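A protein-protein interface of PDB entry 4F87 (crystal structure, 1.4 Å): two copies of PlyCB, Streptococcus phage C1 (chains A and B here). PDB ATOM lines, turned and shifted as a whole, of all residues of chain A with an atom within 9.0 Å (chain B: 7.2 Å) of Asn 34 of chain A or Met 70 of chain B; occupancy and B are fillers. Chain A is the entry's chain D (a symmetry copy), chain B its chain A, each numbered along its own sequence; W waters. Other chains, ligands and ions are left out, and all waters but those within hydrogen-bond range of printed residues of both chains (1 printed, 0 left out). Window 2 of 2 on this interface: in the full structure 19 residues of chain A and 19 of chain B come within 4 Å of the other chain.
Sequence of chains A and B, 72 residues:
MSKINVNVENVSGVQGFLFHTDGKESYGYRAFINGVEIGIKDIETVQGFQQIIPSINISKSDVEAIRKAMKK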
ATOM      1  N   ASN A  10      -8.245  18.120  30.352  1.00  0.00           N
ATOM      2  CA  ASN A  10      -9.699  18.149  30.177  1.00  0.00           C
ATOM      3  C   ASN A  10     -10.055  18.728  28.799  1.00  0.00           C
ATOM      4  O   ASN A  10     -10.984  19.539  28.671  1.00  0.00           O
ATOM      5  CB  ASN A  10     -10.350  18.948  31.314  1.00  0.00           C
ATOM      6  N   VAL A  11      -9.325  18.238  27.761  1.00  0.00           N
ATOM      7  CA  VAL A  11      -9.320  18.638  26.360  1.00  0.00           C
ATOM      8  C   VAL A  11     -10.695  18.746  25.713  1.00  0.00           C
ATOM      9  O   VAL A  11     -10.868  19.644  24.896  1.00  0.00           O
ATOM     10  CB  VAL A  11      -8.347  17.757  25.522  1.00  0.00           C
ATOM     11  CG1 VAL A  11      -8.857  16.319  25.391  1.00  0.00           C
ATOM     12  CG2 VAL A  11      -8.080  18.352  24.161  1.00  0.00           C
ATOM     13  N   SER A  12     -11.633  17.856  26.037  1.00  0.00           N
ATOM     14  CA  SER A  12     -12.939  17.883  25.376  1.00  0.00           C
ATOM     15  C   SER A  12     -13.882  18.978  25.861  1.00  0.00           C
ATOM     16  O   SER A  12     -14.884  19.248  25.188  1.00  0.00           O
ATOM     17  CB  SER A  12     -13.621  16.533  25.504  1.00  0.00           C
ATOM     18  OG  SER A  12     -14.028  16.378  26.858  1.00  0.00           O
ATOM     19  N   GLY A  13     -13.622  19.516  27.043  1.00  0.00           N
ATOM     20  CA  GLY A  13     -14.505  20.496  27.652  1.00  0.00           C
ATOM     21  C   GLY A  13     -15.801  19.840  28.111  1.00  0.00           C
ATOM     22  O   GLY A  13     -16.828  20.513  28.227  1.00  0.00           O
ATOM     23  N   VAL A  14     -15.781  18.500  28.330  1.00  0.00           N
ATOM     24  CA  VAL A  14     -16.968  17.757  28.751  1.00  0.00           C
ATOM     25  C   VAL A  14     -16.622  16.885  29.949  1.00  0.00           C
ATOM     26  O   VAL A  14     -15.684  16.097  29.884  1.00  0.00           O
ATOM     27  CB  VAL A  14     -17.515  16.873  27.610  1.00  0.00           C
ATOM     28  CG1 VAL A  14     -18.732  16.062  28.068  1.00  0.00           C
ATOM     29  CG2 VAL A  14     -17.874  17.710  26.375  1.00  0.00           C
ATOM     30  N   GLN A  15     -17.410  17.006  31.026  1.00  0.00           N
ATOM     31  CA  GLN A  15     -17.298  16.130  32.189  1.00  0.00           C
ATOM     32  C   GLN A  15     -18.660  15.510  32.397  1.00  0.00           C
ATOM     33  O   GLN A  15     -19.657  16.231  32.419  1.00  0.00           O
ATOM     34  CB  GLN A  15     -16.872  16.892  33.439  1.00  0.00           C
ATOM     35  CG  GLN A  15     -15.401  17.289  33.397  1.00  0.00           C
ATOM     36  CD  GLN A  15     -14.968  17.957  34.672  1.00  0.00           C
ATOM     37  OE1 GLN A  15     -15.051  17.384  35.759  1.00  0.00           O
ATOM     38  NE2 GLN A  15     -14.468  19.175  34.562  1.00  0.00           N
ATOM     39  N   GLY A  16     -18.714  14.199  32.572  1.00  0.00           N
ATOM     40  CA  GLY A  16     -19.996  13.541  32.771  1.00  0.00           C
ATOM     41  C   GLY A  16     -19.993  12.097  32.361  1.00  0.00           C
ATOM     42  O   GLY A  16     -18.924  11.488  32.227  1.00  0.00           O
ATOM     43  N   PHE A  17     -21.193  11.555  32.151  1.00  0.00           N
ATOM     44  CA  PHE A  17     -21.309  10.160  31.769  1.00  0.00           C
ATOM     45  C   PHE A  17     -22.635   9.912  31.115  1.00  0.00           C
ATOM     46  O   PHE A  17     -23.611  10.635  31.367  1.00  0.00           O
ATOM     47  CB  PHE A  17     -21.152   9.234  33.023  1.00  0.00           C
ATOM     48  CG  PHE A  17     -22.136   9.508  34.145  1.00  0.00           C
ATOM     49  CD1 PHE A  17     -23.360   8.856  34.191  1.00  0.00           C
ATOM     50  CD2 PHE A  17     -21.815  10.376  35.184  1.00  0.00           C
ATOM     51  CE1 PHE A  17     -24.292   9.122  35.212  1.00  0.00           C
ATOM     52  CE2 PHE A  17     -22.737  10.619  36.223  1.00  0.00           C
ATOM     53  CZ  PHE A  17     -23.955   9.966  36.248  1.00  0.00           C
ATOM     54  N   ALA A  31     -27.649  11.403  29.612  1.00  0.00           N
ATOM     55  CA  ALA A  31     -26.296  11.769  30.026  1.00  0.00           C
ATOM     56  C   ALA A  31     -26.341  12.913  30.970  1.00  0.00           C
ATOM     57  O   ALA A  31     -27.261  13.731  30.922  1.00  0.00           O
ATOM     58  CB  ALA A  31     -25.447  12.175  28.817  1.00  0.00           C
ATOM     59  N   PHE A  32     -25.310  12.992  31.823  1.00  0.00           N
ATOM     60  CA  PHE A  32     -25.008  14.196  32.577  1.00  0.00           C
ATOM     61  C   PHE A  32     -23.813  14.785  31.854  1.00  0.00           C
ATOM     62  O   PHE A  32     -22.792  14.104  31.695  1.00  0.00           O
ATOM     63  CB  PHE A  32     -24.638  13.917  34.039  1.00  0.00           C
ATOM     64  CG  PHE A  32     -25.873  13.714  34.873  1.00  0.00           C
ATOM     65  CD1 PHE A  32     -26.560  14.805  35.408  1.00  0.00           C
ATOM     66  CD2 PHE A  32     -26.353  12.440  35.125  1.00  0.00           C
ATOM     67  CE1 PHE A  32     -27.724  14.608  36.163  1.00  0.00           C
ATOM     68  CE2 PHE A  32     -27.512  12.247  35.890  1.00  0.00           C
ATOM     69  CZ  PHE A  32     -28.201  13.331  36.373  1.00  0.00           C
ATOM     70  N   ILE A  33     -23.957  15.996  31.325  1.00  0.00           N
ATOM     71  CA  ILE A  33     -22.862  16.658  30.620  1.00  0.00           C
ATOM     72  C   ILE A  33     -22.689  18.006  31.294  1.00  0.00           C
ATOM     73  O   ILE A  33     -23.609  18.834  31.271  1.00  0.00           O
ATOM     74  CB  ILE A  33     -23.118  16.765  29.089  1.00  0.00           C
ATOM     75  CG1 ILE A  33     -23.036  15.357  28.413  1.00  0.00           C
ATOM     76  CG2 ILE A  33     -22.119  17.787  28.428  1.00  0.00           C
ATOM     77  CD1 ILE A  33     -23.399  15.280  26.965  1.00  0.00           C
ATOM     78  N   ASN A  34     -21.527  18.216  31.959  1.00  0.00           N
ATOM     79  CA  ASN A  34     -21.238  19.469  32.653  1.00  0.00           C
ATOM     80  C   ASN A  34     -22.356  19.821  33.654  1.00  0.00           C
ATOM     81  O   ASN A  34     -22.772  20.972  33.744  1.00  0.00           O
ATOM     82  CB  ASN A  34     -20.928  20.582  31.623  1.00  0.00           C
ATOM     83  CG  ASN A  34     -19.716  20.265  30.764  1.00  0.00           C
ATOM     84  OD1 ASN A  34     -18.848  19.467  31.146  1.00  0.00           O
ATOM     85  ND2 ASN A  34     -19.583  20.930  29.619  1.00  0.00           N
ATOM     86  N   GLY A  35     -22.875  18.792  34.330  1.00  0.00           N
ATOM     87  CA  GLY A  35     -23.916  18.933  35.343  1.00  0.00           C
ATOM     88  C   GLY A  35     -25.333  19.102  34.830  1.00  0.00           C
ATOM     89  O   GLY A  35     -26.248  19.347  35.625  1.00  0.00           O
ATOM     90  N   VAL A  36     -25.530  18.992  33.503  1.00  0.00           N
ATOM     91  CA  VAL A  36     -26.843  19.139  32.880  1.00  0.00           C
ATOM     92  C   VAL A  36     -27.296  17.771  32.407  1.00  0.00           C
ATOM     93  O   VAL A  36     -26.590  17.117  31.627  1.00  0.00           O
ATOM     94  CB  VAL A  36     -26.799  20.153  31.707  1.00  0.00           C
ATOM     95  CG1 VAL A  36     -28.153  20.250  31.003  1.00  0.00           C
ATOM     96  CG2 VAL A  36     -26.327  21.537  32.185  1.00  0.00           C
ATOM     97  N   GLU A  37     -28.488  17.343  32.834  1.00  0.00           N
ATOM     98  CA  GLU A  37     -29.038  16.075  32.395  1.00  0.00           C
ATOM     99  C   GLU A  37     -29.796  16.251  31.099  1.00  0.00           C
ATOM    100  O   GLU A  37     -30.640  17.144  30.983  1.00  0.00           O
ATOM    101  CB  GLU A  37     -29.965  15.494  33.460  1.00  0.00           C
ATOM    102  CG  GLU A  37     -30.389  14.066  33.142  1.00  0.00           C
ATOM    103  CD  GLU A  37     -31.484  13.545  34.052  1.00  0.00           C
ATOM    104  OE1 GLU A  37     -31.709  14.138  35.133  1.00  0.00           O
ATOM    105  OE2 GLU A  37     -32.169  12.585  33.639  1.00  0.00           O
ATOM    106  N   ILE A  38     -29.507  15.384  30.118  1.00  0.00           N
ATOM    107  CA  ILE A  38     -30.181  15.397  28.812  1.00  0.00           C
ATOM    108  C   ILE A  38     -30.525  13.983  28.369  1.00  0.00           C
ATOM    109  O   ILE A  38     -29.932  13.002  28.841  1.00  0.00           O
ATOM    110  CB  ILE A  38     -29.294  16.068  27.727  1.00  0.00           C
ATOM    111  CG1 ILE A  38     -27.950  15.323  27.554  1.00  0.00           C
ATOM    112  CG2 ILE A  38     -29.127  17.579  28.017  1.00  0.00           C
ATOM    113  CD1 ILE A  38     -27.174  15.738  26.318  1.00  0.00           C
ATOM    114  N   PHE A  49     -20.293  10.213  21.985  1.00  0.00           N
ATOM    115  CA  PHE A  49     -19.898  10.571  23.352  1.00  0.00           C
ATOM    116  C   PHE A  49     -19.142   9.459  24.068  1.00  0.00           C
ATOM    117  O   PHE A  49     -18.318   9.784  24.918  1.00  0.00           O
ATOM    118  CB  PHE A  49     -21.098  11.067  24.172  1.00  0.00           C
ATOM    119  CG  PHE A  49     -21.344  12.529  23.879  1.00  0.00           C
ATOM    120  CD1 PHE A  49     -20.660  13.510  24.574  1.00  0.00           C
ATOM    121  CD2 PHE A  49     -22.143  12.923  22.799  1.00  0.00           C
ATOM    122  CE1 PHE A  49     -20.815  14.860  24.252  1.00  0.00           C
ATOM    123  CE2 PHE A  49     -22.302  14.274  22.489  1.00  0.00           C
ATOM    124  CZ  PHE A  49     -21.622  15.233  23.207  1.00  0.00           C
ATOM    125  N   ILE A  52     -15.453  10.014  24.476  1.00  0.00           N
ATOM    126  CA  ILE A  52     -14.899  11.026  25.385  1.00  0.00           C
ATOM    127  C   ILE A  52     -15.385  10.936  26.825  1.00  0.00           C
ATOM    128  O   ILE A  52     -14.741  11.545  27.687  1.00  0.00           O
ATOM    129  CB  ILE A  52     -15.090  12.459  24.808  1.00  0.00           C
ATOM    130  CG1 ILE A  52     -16.582  12.821  24.584  1.00  0.00           C
ATOM    131  CG2 ILE A  52     -14.255  12.663  23.526  1.00  0.00           C
ATOM    132  CD1 ILE A  52     -16.843  14.349  24.359  1.00  0.00           C
ATOM    133  N   ILE A  53     -16.521  10.279  27.097  1.00  0.00           N
ATOM    134  CA  ILE A  53     -16.991  10.169  28.477  1.00  0.00           C
ATOM    135  C   ILE A  53     -17.368   8.728  28.779  1.00  0.00           C
ATOM    136  O   ILE A  53     -17.743   7.979  27.861  1.00  0.00           O
ATOM    137  CB  ILE A  53     -18.153  11.134  28.827  1.00  0.00           C
ATOM    138  CG1 ILE A  53     -19.373  10.942  27.903  1.00  0.00           C
ATOM    139  CG2 ILE A  53     -17.677  12.587  28.910  1.00  0.00           C
ATOM    140  CD1 ILE A  53     -20.588  11.807  28.276  1.00  0.00           C
ATOM    141  N   MET A  70     -26.240  14.463  41.697  1.00  0.00           N
ATOM    142  CA  MET A  70     -25.621  15.212  40.610  1.00  0.00           C
ATOM    143  C   MET A  70     -26.038  16.696  40.597  1.00  0.00           C
ATOM    144  O   MET A  70     -25.452  17.481  39.844  1.00  0.00           O
ATOM    145  CB  MET A  70     -25.921  14.541  39.253  1.00  0.00           C
ATOM    146  CG  MET A  70     -25.255  13.177  39.056  1.00  0.00           C
ATOM    147  SD  MET A  70     -23.437  13.223  39.165  1.00  0.00           S
ATOM    148  CE  MET A  70     -23.002  14.061  37.602  1.00  0.00           C
ATOM    149  N   GLN B  15     -10.427  23.919  24.646  1.00  0.00           N
ATOM    150  CA  GLN B  15     -11.205  22.803  25.175  1.00  0.00           C
ATOM    151  C   GLN B  15     -12.455  22.686  24.328  1.00  0.00           C
ATOM    152  O   GLN B  15     -13.139  23.682  24.108  1.00  0.00           O
ATOM    153  CB  GLN B  15     -11.597  23.021  26.643  1.00  0.00           C
ATOM    154  CG  GLN B  15     -10.411  22.861  27.579  1.00  0.00           C
ATOM    155  CD  GLN B  15     -10.783  23.092  29.025  1.00  0.00           C
ATOM    156  OE1 GLN B  15     -11.688  22.465  29.564  1.00  0.00           O
ATOM    157  NE2 GLN B  15     -10.072  23.989  29.684  1.00  0.00           N
ATOM    158  N   GLY B  16     -12.741  21.496  23.836  1.00  0.00           N
ATOM    159  CA  GLY B  16     -13.935  21.316  23.020  1.00  0.00           C
ATOM    160  C   GLY B  16     -13.837  20.124  22.113  1.00  0.00           C
ATOM    161  O   GLY B  16     -13.038  19.215  22.349  1.00  0.00           O
ATOM    162  N   PHE B  17     -14.672  20.116  21.067  1.00  0.00           N
ATOM    163  CA  PHE B  17     -14.672  19.004  20.154  1.00  0.00           C
ATOM    164  C   PHE B  17     -15.301  19.423  18.842  1.00  0.00           C
ATOM    165  O   PHE B  17     -16.127  20.343  18.804  1.00  0.00           O
ATOM    166  CB  PHE B  17     -15.446  17.787  20.746  1.00  0.00           C
ATOM    167  CG  PHE B  17     -16.859  18.080  21.194  1.00  0.00           C
ATOM    168  CD1 PHE B  17     -17.924  17.978  20.310  1.00  0.00           C
ATOM    169  CD2 PHE B  17     -17.130  18.454  22.506  1.00  0.00           C
ATOM    170  CE1 PHE B  17     -19.229  18.278  20.722  1.00  0.00           C
ATOM    171  CE2 PHE B  17     -18.447  18.714  22.923  1.00  0.00           C
ATOM    172  CZ  PHE B  17     -19.481  18.621  22.029  1.00  0.00           C
ATOM    173  N   PHE B  32     -17.425  22.937  19.184  1.00  0.00           N
ATOM    174  CA  PHE B  32     -17.507  23.723  20.398  1.00  0.00           C
ATOM    175  C   PHE B  32     -16.061  24.033  20.737  1.00  0.00           C
ATOM    176  O   PHE B  32     -15.250  23.101  20.854  1.00  0.00           O
ATOM    177  CB  PHE B  32     -18.155  22.968  21.576  1.00  0.00           C
ATOM    178  CG  PHE B  32     -19.642  23.002  21.484  1.00  0.00           C
ATOM    179  CD1 PHE B  32     -20.358  24.090  21.961  1.00  0.00           C
ATOM    180  CD2 PHE B  32     -20.335  21.950  20.912  1.00  0.00           C
ATOM    181  CE1 PHE B  32     -21.746  24.124  21.849  1.00  0.00           C
ATOM    182  CE2 PHE B  32     -21.727  21.991  20.797  1.00  0.00           C
ATOM    183  CZ  PHE B  32     -22.410  23.092  21.248  1.00  0.00           C
ATOM    184  N   ILE B  33     -15.708  25.315  20.780  1.00  0.00           N
ATOM    185  CA  ILE B  33     -14.349  25.744  21.126  1.00  0.00           C
ATOM    186  C   ILE B  33     -14.505  26.688  22.320  1.00  0.00           C
ATOM    187  O   ILE B  33     -15.116  27.750  22.174  1.00  0.00           O
ATOM    188  CB  ILE B  33     -13.626  26.484  19.945  1.00  0.00           C
ATOM    189  CG1 ILE B  33     -13.536  25.667  18.634  1.00  0.00           C
ATOM    190  CG2 ILE B  33     -12.234  27.059  20.381  1.00  0.00           C
ATOM    191  CD1 ILE B  33     -12.731  24.466  18.701  1.00  0.00           C
ATOM    192  N   ASN B  34     -13.982  26.286  23.493  1.00  0.00           N
ATOM    193  CA  ASN B  34     -14.064  27.106  24.700  1.00  0.00           C
ATOM    194  C   ASN B  34     -15.508  27.567  24.996  1.00  0.00           C
ATOM    195  O   ASN B  34     -15.743  28.732  25.355  1.00  0.00           O
ATOM    196  CB  ASN B  34     -13.045  28.256  24.612  1.00  0.00           C
ATOM    197  CG  ASN B  34     -11.612  27.750  24.587  1.00  0.00           C
ATOM    198  OD1 ASN B  34     -11.329  26.611  24.988  1.00  0.00           O
ATOM    199  ND2 ASN B  34     -10.665  28.594  24.193  1.00  0.00           N
ATOM    200  N   GLY B  35     -16.452  26.648  24.780  1.00  0.00           N
ATOM    201  CA  GLY B  35     -17.865  26.897  25.031  1.00  0.00           C
ATOM    202  C   GLY B  35     -18.601  27.714  23.988  1.00  0.00           C
ATOM    203  O   GLY B  35     -19.760  28.098  24.214  1.00  0.00           O
ATOM    204  N   VAL B  36     -17.952  27.984  22.842  1.00  0.00           N
ATOM    205  CA  VAL B  36     -18.560  28.729  21.744  1.00  0.00           C
ATOM    206  C   VAL B  36     -18.762  27.773  20.584  1.00  0.00           C
ATOM    207  O   VAL B  36     -17.811  27.148  20.115  1.00  0.00           O
ATOM    208  CB  VAL B  36     -17.690  29.960  21.343  1.00  0.00           C
ATOM    209  CG1 VAL B  36     -18.286  30.704  20.142  1.00  0.00           C
ATOM    210  CG2 VAL B  36     -17.509  30.913  22.535  1.00  0.00           C
ATOM    211  N   GLU B  37     -19.996  27.692  20.093  1.00  0.00           N
ATOM    212  CA  GLU B  37     -20.299  26.853  18.952  1.00  0.00           C
ATOM    213  C   GLU B  37     -20.059  27.607  17.663  1.00  0.00           C
ATOM    214  O   GLU B  37     -20.516  28.752  17.505  1.00  0.00           O
ATOM    215  CB  GLU B  37     -21.739  26.369  19.007  1.00  0.00           C
ATOM    216  CG  GLU B  37     -22.044  25.319  17.951  1.00  0.00           C
ATOM    217  CD  GLU B  37     -23.514  25.014  17.822  1.00  0.00           C
ATOM    218  OE1 GLU B  37     -24.273  25.327  18.770  1.00  0.00           O
ATOM    219  OE2 GLU B  37     -23.911  24.479  16.762  1.00  0.00           O
ATOM    220  N   GLU B  64     -29.528  19.931  19.541  1.00  0.00           N
ATOM    221  CA  GLU B  64     -30.211  20.870  20.445  1.00  0.00           C
ATOM    222  C   GLU B  64     -29.918  20.550  21.933  1.00  0.00           C
ATOM    223  O   GLU B  64     -29.586  21.457  22.714  1.00  0.00           O
ATOM    224  CB  GLU B  64     -31.716  20.858  20.165  1.00  0.00           C
ATOM    225  CG  GLU B  64     -32.524  21.817  21.024  1.00  0.00           C
ATOM    226  CD  GLU B  64     -33.994  21.899  20.657  1.00  0.00           C
ATOM    227  OE1 GLU B  64     -34.505  23.035  20.552  1.00  0.00           O
ATOM    228  OE2 GLU B  64     -34.629  20.838  20.456  1.00  0.00           O
ATOM    229  N   ALA B  65     -29.985  19.275  22.310  1.00  0.00           N
ATOM    230  CA  ALA B  65     -29.717  18.908  23.706  1.00  0.00           C
ATOM    231  C   ALA B  65     -28.254  19.114  24.073  1.00  0.00           C
ATOM    232  O   ALA B  65     -27.960  19.556  25.187  1.00  0.00           O
ATOM    233  CB  ALA B  65     -30.113  17.465  23.940  1.00  0.00           C
ATOM    234  N   ILE B  66     -27.322  18.832  23.135  1.00  0.00           N
ATOM    235  CA  ILE B  66     -25.906  19.030  23.425  1.00  0.00           C
ATOM    236  C   ILE B  66     -25.631  20.527  23.613  1.00  0.00           C
ATOM    237  O   ILE B  66     -24.886  20.897  24.511  1.00  0.00           O
ATOM    238  CB  ILE B  66     -25.003  18.394  22.335  1.00  0.00           C
ATOM    239  CG1 ILE B  66     -25.250  16.881  22.176  1.00  0.00           C
ATOM    240  CG2 ILE B  66     -23.518  18.709  22.570  1.00  0.00           C
ATOM    241  CD1 ILE B  66     -25.151  16.067  23.469  1.00  0.00           C
ATOM    242  N   ARG B  67     -26.278  21.389  22.804  1.00  0.00           N
ATOM    243  CA  ARG B  67     -26.127  22.835  22.967  1.00  0.00           C
ATOM    244  C   ARG B  67     -26.533  23.254  24.360  1.00  0.00           C
ATOM    245  O   ARG B  67     -25.837  24.073  24.953  1.00  0.00           O
ATOM    246  CB  ARG B  67     -27.058  23.554  22.012  1.00  0.00           C
ATOM    247  CG  ARG B  67     -26.540  23.587  20.642  1.00  0.00           C
ATOM    248  CD  ARG B  67     -27.444  24.441  19.803  1.00  0.00           C
ATOM    249  NE  ARG B  67     -26.842  24.541  18.494  1.00  0.00           N
ATOM    250  CZ  ARG B  67     -27.455  24.303  17.348  1.00  0.00           C
ATOM    251  NH1 ARG B  67     -28.767  24.070  17.321  1.00  0.00           N
ATOM    252  NH2 ARG B  67     -26.779  24.347  16.214  1.00  0.00           N
ATOM    253  N   LYS B  68     -27.652  22.701  24.883  1.00  0.00           N
ATOM    254  CA  LYS B  68     -28.162  23.027  26.223  1.00  0.00           C
ATOM    255  C   LYS B  68     -27.114  22.653  27.278  1.00  0.00           C
ATOM    256  O   LYS B  68     -26.834  23.452  28.180  1.00  0.00           O
ATOM    257  CB  LYS B  68     -29.492  22.282  26.475  1.00  0.00           C
ATOM    258  CG  LYS B  68     -30.158  22.617  27.811  1.00  0.00           C
ATOM    259  CD  LYS B  68     -31.390  21.760  28.051  1.00  0.00           C
ATOM    260  N   ALA B  69     -26.514  21.459  27.147  1.00  0.00           N
ATOM    261  CA  ALA B  69     -25.504  20.987  28.090  1.00  0.00           C
ATOM    262  C   ALA B  69     -24.178  21.733  28.006  1.00  0.00           C
ATOM    263  O   ALA B  69     -23.484  21.871  29.021  1.00  0.00           O
ATOM    264  CB  ALA B  69     -25.286  19.496  27.908  1.00  0.00           C
ATOM    265  N   MET B  70     -23.827  22.244  26.812  1.00  0.00           N
ATOM    266  CA  MET B  70     -22.576  22.944  26.594  1.00  0.00           C
ATOM    267  C   MET B  70     -22.670  24.428  26.979  1.00  0.00           C
ATOM    268  O   MET B  70     -21.636  25.088  27.037  1.00  0.00           O
ATOM    269  CB  MET B  70     -22.086  22.761  25.149  1.00  0.00           C
ATOM    270  CG  MET B  70     -21.661  21.330  24.802  1.00  0.00           C
ATOM    271  SD  MET B  70     -20.313  20.650  25.848  1.00  0.00           S
ATOM    272  CE  MET B  70     -18.904  21.619  25.152  1.00  0.00           C
ATOM    273  N   LYS B  71     -23.894  24.939  27.254  1.00  0.00           N
ATOM    274  CA  LYS B  71     -24.163  26.351  27.586  1.00  0.00           C
ATOM    275  C   LYS B  71     -23.399  26.854  28.815  1.00  0.00           C
ATOM    276  O   LYS B  71     -23.179  26.105  29.761  1.00  0.00           O
ATOM    277  CB  LYS B  71     -25.674  26.592  27.745  1.00  0.00           C
ATOM    278  CG  LYS B  71     -26.088  28.057  27.651  1.00  0.00           C
HETATM  279  O   HOH W   1     -20.766  23.471  29.595  1.00  0.00           O
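The backbone carbonyl oxygen of Ser 12 of chain A lies close to the backbone NH of Gly 16 of chain B (3.4 Å). The backbone NH (N) of Gly 16 of chain B sits at hydrogen-bond distance from the backbone carbonyl oxygen (O) of Val 11 of chain A, 2.8 Å away. The backbone carbonyl oxygen of Asn 10 of chain A lies close to the side-chain amide oxygen of Gln 15 of chain B (3.1 Å).
Of the 17 printed residues of chain B, 7 touch a printed residue of chain A. Of the 20 printed residues of chain A, 10 touch a printed residue of chain B. Printed residues of chain A that touch a printed residue of chain B: Asn 10, Val 11, Ser 12, Gly 13, Val 14, Ile 33, Asn 34, Val 36, Ile 38 and Phe 49. Hydrophobic or aromatic side chains of chain A that line the printed part of chain B: Val 14, Ile 33, Val 36, Ile 38 and Phe 49.
Asn 34 of chain A touches Met 70 of chain B, but with the chains exchanged Met 70 of chain A does not touch Asn 34 of chain B (19.9 Å). Positions printed for both chains: 15, 16, 17, 32, 33, 34, 35, 36, 37 and 70.
Of the printed residues of chain B, Ser 12 of chain A touches Gly 16 and Phe 17. Of chain B, only Ala 69 (3.9 Å) and Met 70 (3.9 Å) come within 4 Å of Asn 34 of chain A. Of the printed residues of chain A, Gln 15 of chain B touches Asn 10, Val 11 and Gly 13. Ile 33 of chain B touches none of the printed residues of chain A. Val 36 of chain B touches none of the printed residues of chain A. Met 70 of chain B touches just these residues of chain A: Gly 13 (3.9 Å), Val 14 (3.9 Å) and Asn 34 (3.9 Å). The nearest printed residue of chain B that does not touch Phe 49 of chain A is Phe 17 of chain B (4.2 Å).
O of Gly 13 of chain A lies within hydrogen-bond range of ND2 of Asn 34 of chain A, at 3.1 Å. O of Ile 38 of chain A lies within hydrogen-bond range of N of Ala 31 of chain A. N of Phe 32 of chain B lies within hydrogen-bond range of O of Phe 17 of chain B (2.9 Å). The backbone NH (N) of Asn 34 of chain A sits at hydrogen-bond distance from the backbone carbonyl oxygen (O) of Gln 15 of chain A, 2.8 Å away. The side-chain hydroxyl (OG) of Ser 12 of chain A lies within hydrogen-bond range of the backbone NH (N) of Val 14 of chain A. The backbone NH (N) of Asn 34 of chain B sits at hydrogen-bond distance from the backbone carbonyl oxygen (O) of Gln 15 of chain B (2.8 Å).
Water W1 lies within hydrogen-bond range of the side-chain amide nitrogen of Asn 34 of chain A (2.8 Å), the backbone carbonyl oxygen of Met 70 of chain B (3.1 Å) and the backbone carbonyl oxygen of Ala 69 of chain B (3.2 Å).
Among the printed residues, merely in contact across the chains: Val 11 of chain A with Gln 15 of chain B (3.2 Å), Phe 49 of chain A with Ile 66 of chain B (3.5 Å), Ile 38 of chain A with Ile 66 of chain B (3.5 Å), Ser 12 of chain A with Phe 17 of chain B (3.6 Å), Ile 33 of chain A with Ala 69 of chain B (3.6 Å), Val 14 of chain A with Phe 17 of chain B (3.6 Å), Ile 38 of chain A with Ala 65 of chain B (3.6 Å), Asn 34 of chain A with Met 70 of chain B (3.9 Å), Val 14 of chain A with Met 70 of chain B (3.9 Å), Asn 34 of chain A with Ala 69 of chain B (3.9 Å), Gly 13 of chain A with Gly 16 of chain B (3.9 Å), Gly 13 of chain A with Met 70 of chain B (3.9 Å), Val 36 of chain A with Ala 69 of chain B (3.9 Å), Gly 13 of chain A with Gln 15 of chain B (3.9 Å) and Ile 33 of chain A with Ile 66 of chain B (3.99 Å).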
